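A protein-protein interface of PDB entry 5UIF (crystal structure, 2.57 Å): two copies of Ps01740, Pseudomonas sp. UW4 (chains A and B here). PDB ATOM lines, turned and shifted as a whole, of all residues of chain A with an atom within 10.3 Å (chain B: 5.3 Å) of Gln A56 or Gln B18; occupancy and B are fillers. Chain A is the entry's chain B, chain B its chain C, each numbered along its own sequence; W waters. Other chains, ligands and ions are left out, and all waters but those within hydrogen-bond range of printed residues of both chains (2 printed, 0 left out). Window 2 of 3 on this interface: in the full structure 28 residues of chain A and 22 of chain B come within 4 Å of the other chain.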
ATOM      1  N   VAL A   8      29.482  30.753 -20.565  1.00  0.00           N
ATOM      2  CA  VAL A   8      28.445  29.730 -20.634  1.00  0.00           C
ATOM      3  C   VAL A   8      28.301  29.268 -22.082  1.00  0.00           C
ATOM      4  O   VAL A   8      28.337  30.085 -23.002  1.00  0.00           O
ATOM      5  CB  VAL A   8      27.092  30.253 -20.100  1.00  0.00           C
ATOM      6  CG1 VAL A   8      25.987  29.230 -20.323  1.00  0.00           C
ATOM      7  CG2 VAL A   8      27.204  30.608 -18.623  1.00  0.00           C
ATOM      8  N   PRO A  48      25.162  25.302 -19.149  1.00  0.00           N
ATOM      9  CA  PRO A  48      24.176  26.177 -18.505  1.00  0.00           C
ATOM     10  C   PRO A  48      23.633  25.551 -17.224  1.00  0.00           C
ATOM     11  O   PRO A  48      23.084  24.450 -17.260  1.00  0.00           O
ATOM     12  CB  PRO A  48      23.078  26.318 -19.566  1.00  0.00           C
ATOM     13  CG  PRO A  48      23.243  25.128 -20.449  1.00  0.00           C
ATOM     14  CD  PRO A  48      24.714  24.841 -20.473  1.00  0.00           C
ATOM     15  N   GLY A  49      23.797  26.248 -16.107  1.00  0.00           N
ATOM     16  CA  GLY A  49      23.404  25.717 -14.816  1.00  0.00           C
ATOM     17  C   GLY A  49      24.616  25.290 -14.012  1.00  0.00           C
ATOM     18  O   GLY A  49      24.494  24.844 -12.871  1.00  0.00           O
ATOM     19  N   SER A  50      25.792  25.422 -14.617  1.00  0.00           N
ATOM     20  CA  SER A  50      27.046  25.113 -13.940  1.00  0.00           C
ATOM     21  C   SER A  50      27.846  26.388 -13.697  1.00  0.00           C
ATOM     22  O   SER A  50      28.978  26.343 -13.215  1.00  0.00           O
ATOM     23  CB  SER A  50      27.869  24.113 -14.754  1.00  0.00           C
ATOM     24  OG  SER A  50      27.195  22.871 -14.868  1.00  0.00           O
ATOM     25  N   ALA A  51      27.247  27.524 -14.038  1.00  0.00           N
ATOM     26  CA  ALA A  51      27.857  28.826 -13.795  1.00  0.00           C
ATOM     27  C   ALA A  51      26.967  29.650 -12.870  1.00  0.00           C
ATOM     28  O   ALA A  51      25.778  29.827 -13.134  1.00  0.00           O
ATOM     29  CB  ALA A  51      28.095  29.559 -15.105  1.00  0.00           C
ATOM     30  N   PHE A  52      27.546  30.151 -11.784  1.00  0.00           N
ATOM     31  CA  PHE A  52      26.771  30.865 -10.778  1.00  0.00           C
ATOM     32  C   PHE A  52      27.359  32.232 -10.446  1.00  0.00           C
ATOM     33  O   PHE A  52      28.575  32.398 -10.369  1.00  0.00           O
ATOM     34  CB  PHE A  52      26.666  30.030  -9.497  1.00  0.00           C
ATOM     35  CG  PHE A  52      25.837  28.786  -9.646  1.00  0.00           C
ATOM     36  CD1 PHE A  52      26.387  27.628 -10.173  1.00  0.00           C
ATOM     37  CD2 PHE A  52      24.510  28.769  -9.249  1.00  0.00           C
ATOM     38  CE1 PHE A  52      25.628  26.481 -10.308  1.00  0.00           C
ATOM     39  CE2 PHE A  52      23.746  27.625  -9.380  1.00  0.00           C
ATOM     40  CZ  PHE A  52      24.306  26.479  -9.911  1.00  0.00           C
ATOM     41  N   THR A  53      26.477  33.208 -10.261  1.00  0.00           N
ATOM     42  CA  THR A  53      26.853  34.514  -9.738  1.00  0.00           C
ATOM     43  C   THR A  53      25.963  34.786  -8.533  1.00  0.00           C
ATOM     44  O   THR A  53      24.780  34.442  -8.550  1.00  0.00           O
ATOM     45  CB  THR A  53      26.705  35.631 -10.788  1.00  0.00           C
ATOM     46  OG1 THR A  53      27.481  35.305 -11.948  1.00  0.00           O
ATOM     47  CG2 THR A  53      27.178  36.965 -10.230  1.00  0.00           C
ATOM     48  N   ALA A  54      26.534  35.397  -7.496  1.00  0.00           N
ATOM     49  CA  ALA A  54      25.890  35.479  -6.189  1.00  0.00           C
ATOM     50  C   ALA A  54      25.521  34.072  -5.737  1.00  0.00           C
ATOM     51  O   ALA A  54      26.397  33.255  -5.463  1.00  0.00           O
ATOM     52  CB  ALA A  54      24.663  36.386  -6.227  1.00  0.00           C
ATOM     53  N   GLY A  55      24.228  33.779  -5.690  1.00  0.00           N
ATOM     54  CA  GLY A  55      23.782  32.455  -5.300  1.00  0.00           C
ATOM     55  C   GLY A  55      23.094  31.697  -6.418  1.00  0.00           C
ATOM     56  O   GLY A  55      22.898  30.485  -6.325  1.00  0.00           O
ATOM     57  N   GLN A  56      22.739  32.405  -7.485  1.00  0.00           N
ATOM     58  CA  GLN A  56      21.912  31.825  -8.538  1.00  0.00           C
ATOM     59  C   GLN A  56      22.650  31.640  -9.860  1.00  0.00           C
ATOM     60  O   GLN A  56      23.774  32.114 -10.032  1.00  0.00           O
ATOM     61  CB  GLN A  56      20.672  32.692  -8.759  1.00  0.00           C
ATOM     62  CG  GLN A  56      19.893  32.973  -7.487  1.00  0.00           C
ATOM     63  CD  GLN A  56      19.532  31.705  -6.739  1.00  0.00           C
ATOM     64  OE1 GLN A  56      19.149  30.703  -7.342  1.00  0.00           O
ATOM     65  NE2 GLN A  56      19.663  31.740  -5.417  1.00  0.00           N
ATOM     66  N   VAL A  57      22.001  30.944 -10.787  1.00  0.00           N
ATOM     67  CA  VAL A  57      22.556  30.705 -12.114  1.00  0.00           C
ATOM     68  C   VAL A  57      22.629  32.001 -12.912  1.00  0.00           C
ATOM     69  O   VAL A  57      21.650  32.742 -13.002  1.00  0.00           O
ATOM     70  CB  VAL A  57      21.721  29.673 -12.902  1.00  0.00           C
ATOM     71  CG1 VAL A  57      22.287  29.484 -14.302  1.00  0.00           C
ATOM     72  CG2 VAL A  57      21.674  28.347 -12.162  1.00  0.00           C
ATOM     73  N   ALA A  58      23.795  32.272 -13.486  1.00  0.00           N
ATOM     74  CA  ALA A  58      23.983  33.464 -14.299  1.00  0.00           C
ATOM     75  C   ALA A  58      24.898  33.171 -15.480  1.00  0.00           C
ATOM     76  O   ALA A  58      25.237  32.018 -15.745  1.00  0.00           O
ATOM     77  CB  ALA A  58      24.545  34.593 -13.457  1.00  0.00           C
ATOM     78  N   THR A  59      25.296  34.222 -16.190  1.00  0.00           N
ATOM     79  CA  THR A  59      26.189  34.073 -17.332  1.00  0.00           C
ATOM     80  C   THR A  59      27.399  34.999 -17.239  1.00  0.00           C
ATOM     81  O   THR A  59      27.549  35.909 -18.053  1.00  0.00           O
ATOM     82  CB  THR A  59      25.454  34.353 -18.657  1.00  0.00           C
ATOM     83  OG1 THR A  59      24.798  35.624 -18.581  1.00  0.00           O
ATOM     84  CG2 THR A  59      24.420  33.272 -18.933  1.00  0.00           C
ATOM     85  N   PRO A  60      28.275  34.766 -16.247  1.00  0.00           N
ATOM     86  CA  PRO A  60      29.462  35.617 -16.129  1.00  0.00           C
ATOM     87  C   PRO A  60      30.480  35.306 -17.220  1.00  0.00           C
ATOM     88  O   PRO A  60      30.354  34.294 -17.909  1.00  0.00           O
ATOM     89  CB  PRO A  60      30.009  35.257 -14.747  1.00  0.00           C
ATOM     90  CG  PRO A  60      29.611  33.836 -14.565  1.00  0.00           C
ATOM     91  CD  PRO A  60      28.269  33.690 -15.239  1.00  0.00           C
ATOM     92  N   SER B  13      24.958  16.362  -8.672  1.00  0.00           N
ATOM     93  CA  SER B  13      23.643  16.574  -9.257  1.00  0.00           C
ATOM     94  C   SER B  13      23.375  18.071  -9.320  1.00  0.00           C
ATOM     95  O   SER B  13      24.146  18.865  -8.783  1.00  0.00           O
ATOM     96  CB  SER B  13      22.562  15.861  -8.443  1.00  0.00           C
ATOM     97  OG  SER B  13      22.480  16.389  -7.132  1.00  0.00           O
ATOM     98  N   GLU B  14      22.287  18.455  -9.981  1.00  0.00           N
ATOM     99  CA  GLU B  14      21.932  19.865 -10.097  1.00  0.00           C
ATOM    100  C   GLU B  14      21.654  20.471  -8.726  1.00  0.00           C
ATOM    101  O   GLU B  14      22.023  21.613  -8.454  1.00  0.00           O
ATOM    102  CB  GLU B  14      20.718  20.043 -11.010  1.00  0.00           C
ATOM    103  CG  GLU B  14      20.195  21.469 -11.067  1.00  0.00           C
ATOM    104  CD  GLU B  14      18.873  21.579 -11.798  1.00  0.00           C
ATOM    105  OE1 GLU B  14      17.836  21.741 -11.122  1.00  0.00           O
ATOM    106  OE2 GLU B  14      18.867  21.510 -13.046  1.00  0.00           O
ATOM    107  N   ARG B  15      21.007  19.691  -7.865  1.00  0.00           N
ATOM    108  CA  ARG B  15      20.667  20.142  -6.521  1.00  0.00           C
ATOM    109  C   ARG B  15      21.931  20.348  -5.691  1.00  0.00           C
ATOM    110  O   ARG B  15      22.033  21.311  -4.926  1.00  0.00           O
ATOM    111  CB  ARG B  15      19.732  19.137  -5.838  1.00  0.00           C
ATOM    112  CG  ARG B  15      19.957  18.981  -4.337  1.00  0.00           C
ATOM    113  CD  ARG B  15      19.336  17.702  -3.783  1.00  0.00           C
ATOM    114  NE  ARG B  15      20.186  16.538  -4.003  1.00  0.00           N
ATOM    115  CZ  ARG B  15      21.294  16.277  -3.318  1.00  0.00           C
ATOM    116  NH1 ARG B  15      21.698  17.100  -2.357  1.00  0.00           N
ATOM    117  NH2 ARG B  15      22.002  15.190  -3.596  1.00  0.00           N
ATOM    118  N   GLN B  16      22.896  19.445  -5.853  1.00  0.00           N
ATOM    119  CA  GLN B  16      24.172  19.556  -5.150  1.00  0.00           C
ATOM    120  C   GLN B  16      24.978  20.754  -5.646  1.00  0.00           C
ATOM    121  O   GLN B  16      25.637  21.436  -4.858  1.00  0.00           O
ATOM    122  CB  GLN B  16      24.988  18.271  -5.308  1.00  0.00           C
ATOM    123  CG  GLN B  16      24.423  17.084  -4.548  1.00  0.00           C
ATOM    124  CD  GLN B  16      25.240  15.823  -4.740  1.00  0.00           C
ATOM    125  OE1 GLN B  16      25.421  15.350  -5.861  1.00  0.00           O
ATOM    126  NE2 GLN B  16      25.736  15.268  -3.639  1.00  0.00           N
ATOM    127  N   ARG B  17      24.928  21.004  -6.952  1.00  0.00           N
ATOM    128  CA  ARG B  17      25.601  22.162  -7.528  1.00  0.00           C
ATOM    129  C   ARG B  17      25.002  23.450  -6.978  1.00  0.00           C
ATOM    130  O   ARG B  17      25.725  24.361  -6.575  1.00  0.00           O
ATOM    131  CB  ARG B  17      25.509  22.148  -9.055  1.00  0.00           C
ATOM    132  CG  ARG B  17      26.530  21.252  -9.731  1.00  0.00           C
ATOM    133  CD  ARG B  17      26.634  21.568 -11.213  1.00  0.00           C
ATOM    134  NE  ARG B  17      25.359  21.395 -11.901  1.00  0.00           N
ATOM    135  CZ  ARG B  17      24.940  20.244 -12.416  1.00  0.00           C
ATOM    136  NH1 ARG B  17      25.699  19.161 -12.321  1.00  0.00           N
ATOM    137  NH2 ARG B  17      23.765  20.175 -13.025  1.00  0.00           N
ATOM    138  N   GLN B  18      23.674  23.510  -6.960  1.00  0.00           N
ATOM    139  CA  GLN B  18      22.960  24.659  -6.421  1.00  0.00           C
ATOM    140  C   GLN B  18      23.316  24.878  -4.955  1.00  0.00           C
ATOM    141  O   GLN B  18      23.535  26.010  -4.520  1.00  0.00           O
ATOM    142  CB  GLN B  18      21.449  24.470  -6.574  1.00  0.00           C
ATOM    143  CG  GLN B  18      20.620  25.629  -6.050  1.00  0.00           C
ATOM    144  CD  GLN B  18      20.810  26.895  -6.861  1.00  0.00           C
ATOM    145  OE1 GLN B  18      20.967  26.846  -8.081  1.00  0.00           O
ATOM    146  NE2 GLN B  18      20.800  28.038  -6.186  1.00  0.00           N
ATOM    147  N   SER B  19      23.378  23.785  -4.201  1.00  0.00           N
ATOM    148  CA  SER B  19      23.720  23.839  -2.785  1.00  0.00           C
ATOM    149  C   SER B  19      25.136  24.360  -2.575  1.00  0.00           C
ATOM    150  O   SER B  19      25.354  25.297  -1.806  1.00  0.00           O
ATOM    151  CB  SER B  19      23.569  22.458  -2.144  1.00  0.00           C
ATOM    152  OG  SER B  19      24.006  22.470  -0.797  1.00  0.00           O
ATOM    153  N   LEU B  20      26.095  23.749  -3.266  1.00  0.00           N
ATOM    154  CA  LEU B  20      27.496  24.141  -3.152  1.00  0.00           C
ATOM    155  C   LEU B  20      27.712  25.594  -3.562  1.00  0.00           C
ATOM    156  O   LEU B  20      28.511  26.303  -2.955  1.00  0.00           O
ATOM    157  CB  LEU B  20      28.381  23.221  -3.996  1.00  0.00           C
ATOM    158  CG  LEU B  20      28.603  21.806  -3.458  1.00  0.00           C
ATOM    159  CD1 LEU B  20      29.358  20.954  -4.469  1.00  0.00           C
ATOM    160  CD2 LEU B  20      29.348  21.856  -2.134  1.00  0.00           C
ATOM    161  N   ALA B  21      26.993  26.035  -4.591  1.00  0.00           N
ATOM    162  CA  ALA B  21      27.120  27.402  -5.083  1.00  0.00           C
ATOM    163  C   ALA B  21      26.654  28.417  -4.043  1.00  0.00           C
ATOM    164  O   ALA B  21      27.349  29.394  -3.764  1.00  0.00           O
ATOM    165  CB  ALA B  21      26.338  27.573  -6.374  1.00  0.00           C
ATOM    166  N   GLU B  22      25.477  28.179  -3.473  1.00  0.00           N
ATOM    167  CA  GLU B  22      24.925  29.064  -2.452  1.00  0.00           C
ATOM    168  C   GLU B  22      25.787  29.063  -1.193  1.00  0.00           C
ATOM    169  O   GLU B  22      25.957  30.095  -0.543  1.00  0.00           O
ATOM    170  CB  GLU B  22      23.493  28.656  -2.100  1.00  0.00           C
ATOM    171  CG  GLU B  22      22.495  28.812  -3.237  1.00  0.00           C
ATOM    172  CD  GLU B  22      21.086  28.422  -2.831  1.00  0.00           C
ATOM    173  OE1 GLU B  22      20.605  27.362  -3.283  1.00  0.00           O
ATOM    174  OE2 GLU B  22      20.460  29.176  -2.056  1.00  0.00           O
ATOM    175  N   SER B  23      26.329  27.896  -0.858  1.00  0.00           N
ATOM    176  CA  SER B  23      27.146  27.742   0.339  1.00  0.00           C
ATOM    177  C   SER B  23      28.505  28.420   0.190  1.00  0.00           C
ATOM    178  O   SER B  23      28.905  29.208   1.046  1.00  0.00           O
ATOM    179  CB  SER B  23      27.333  26.261   0.670  1.00  0.00           C
ATOM    180  OG  SER B  23      26.085  25.626   0.889  1.00  0.00           O
HETATM  181  O   HOH W   1      19.995  28.531  -9.517  1.00  0.00           O
HETATM  182  O   HOH W   2      25.040  21.855 -15.673  1.00  0.00           O
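NE2 of Gln B18 lies within hydrogen-bond range of O of Gly A55, 3.2 Å away.
The side-chain amide nitrogen (NE2) of Gln B18 sits at hydrogen-bond distance from the side-chain amide oxygen (OE1) of Gln A56, at 3.3 Å.
The side-chain carboxylate of Glu B22 lies within hydrogen-bond range of the side-chain amide nitrogen of Gln B18 (3.0 Å).
Among the printed residues, merely in contact across the chains: Phe A52 with Gln B18, Phe A52 with Ala B21, Gly A55 with Glu B22, Gly A49 with Arg B17 and Ser A50 with Arg B17.
Gln A56 touches just one residue of chain B: Gln B18 (3.3 Å).
Of chain A, only Phe A52, Gly A55 and Gln A56 come within 4 Å of Gln B18.
No residue of chain A comes within 4 Å of Ser B19.
Ala B21 touches just one residue of chain A: Phe A52.
Printed residues of chain B within 4 Å of Gly A49: Arg B17.
Printed residues of chain B within 4 Å of Phe A52: Gln B18 and Ala B21.
Of the printed residues of chain B, Gly A55 touches Gln B18 (3.2 Å) and Glu B22 (3.5 Å).
Of the printed residues of chain B, Ser A50 touches Arg B17 (3.8 Å).
The nearest printed residue of chain B that does not touch Gly A55 is Ala B21 (4.5 Å).
Of the 11 printed residues of chain B, 4 touch a printed residue of chain A.
Printed residues of chain B that touch a printed residue of chain A: Arg B17, Gln B18, Ala B21 and Glu B22.
Of the 14 printed residues of chain A, 5 touch a printed residue of chain B.
Hydrophobic or aromatic side chains of chain A within 4 Å of the printed part of chain B: Phe A52.
No position is printed for both chains.
Water W1 lies within hydrogen-bond range of the side-chain amide oxygen (OE1) of Gln B18 (2.4 Å), the side-chain amide oxygen (OE1) of Gln A56 (3.2 Å) and the backbone NH (N) of Val A57 (3.4 Å).
Water W2 bridges OG of Ser A50 (2.5 Å) and NH2 of Arg B17 (3.4 Å).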
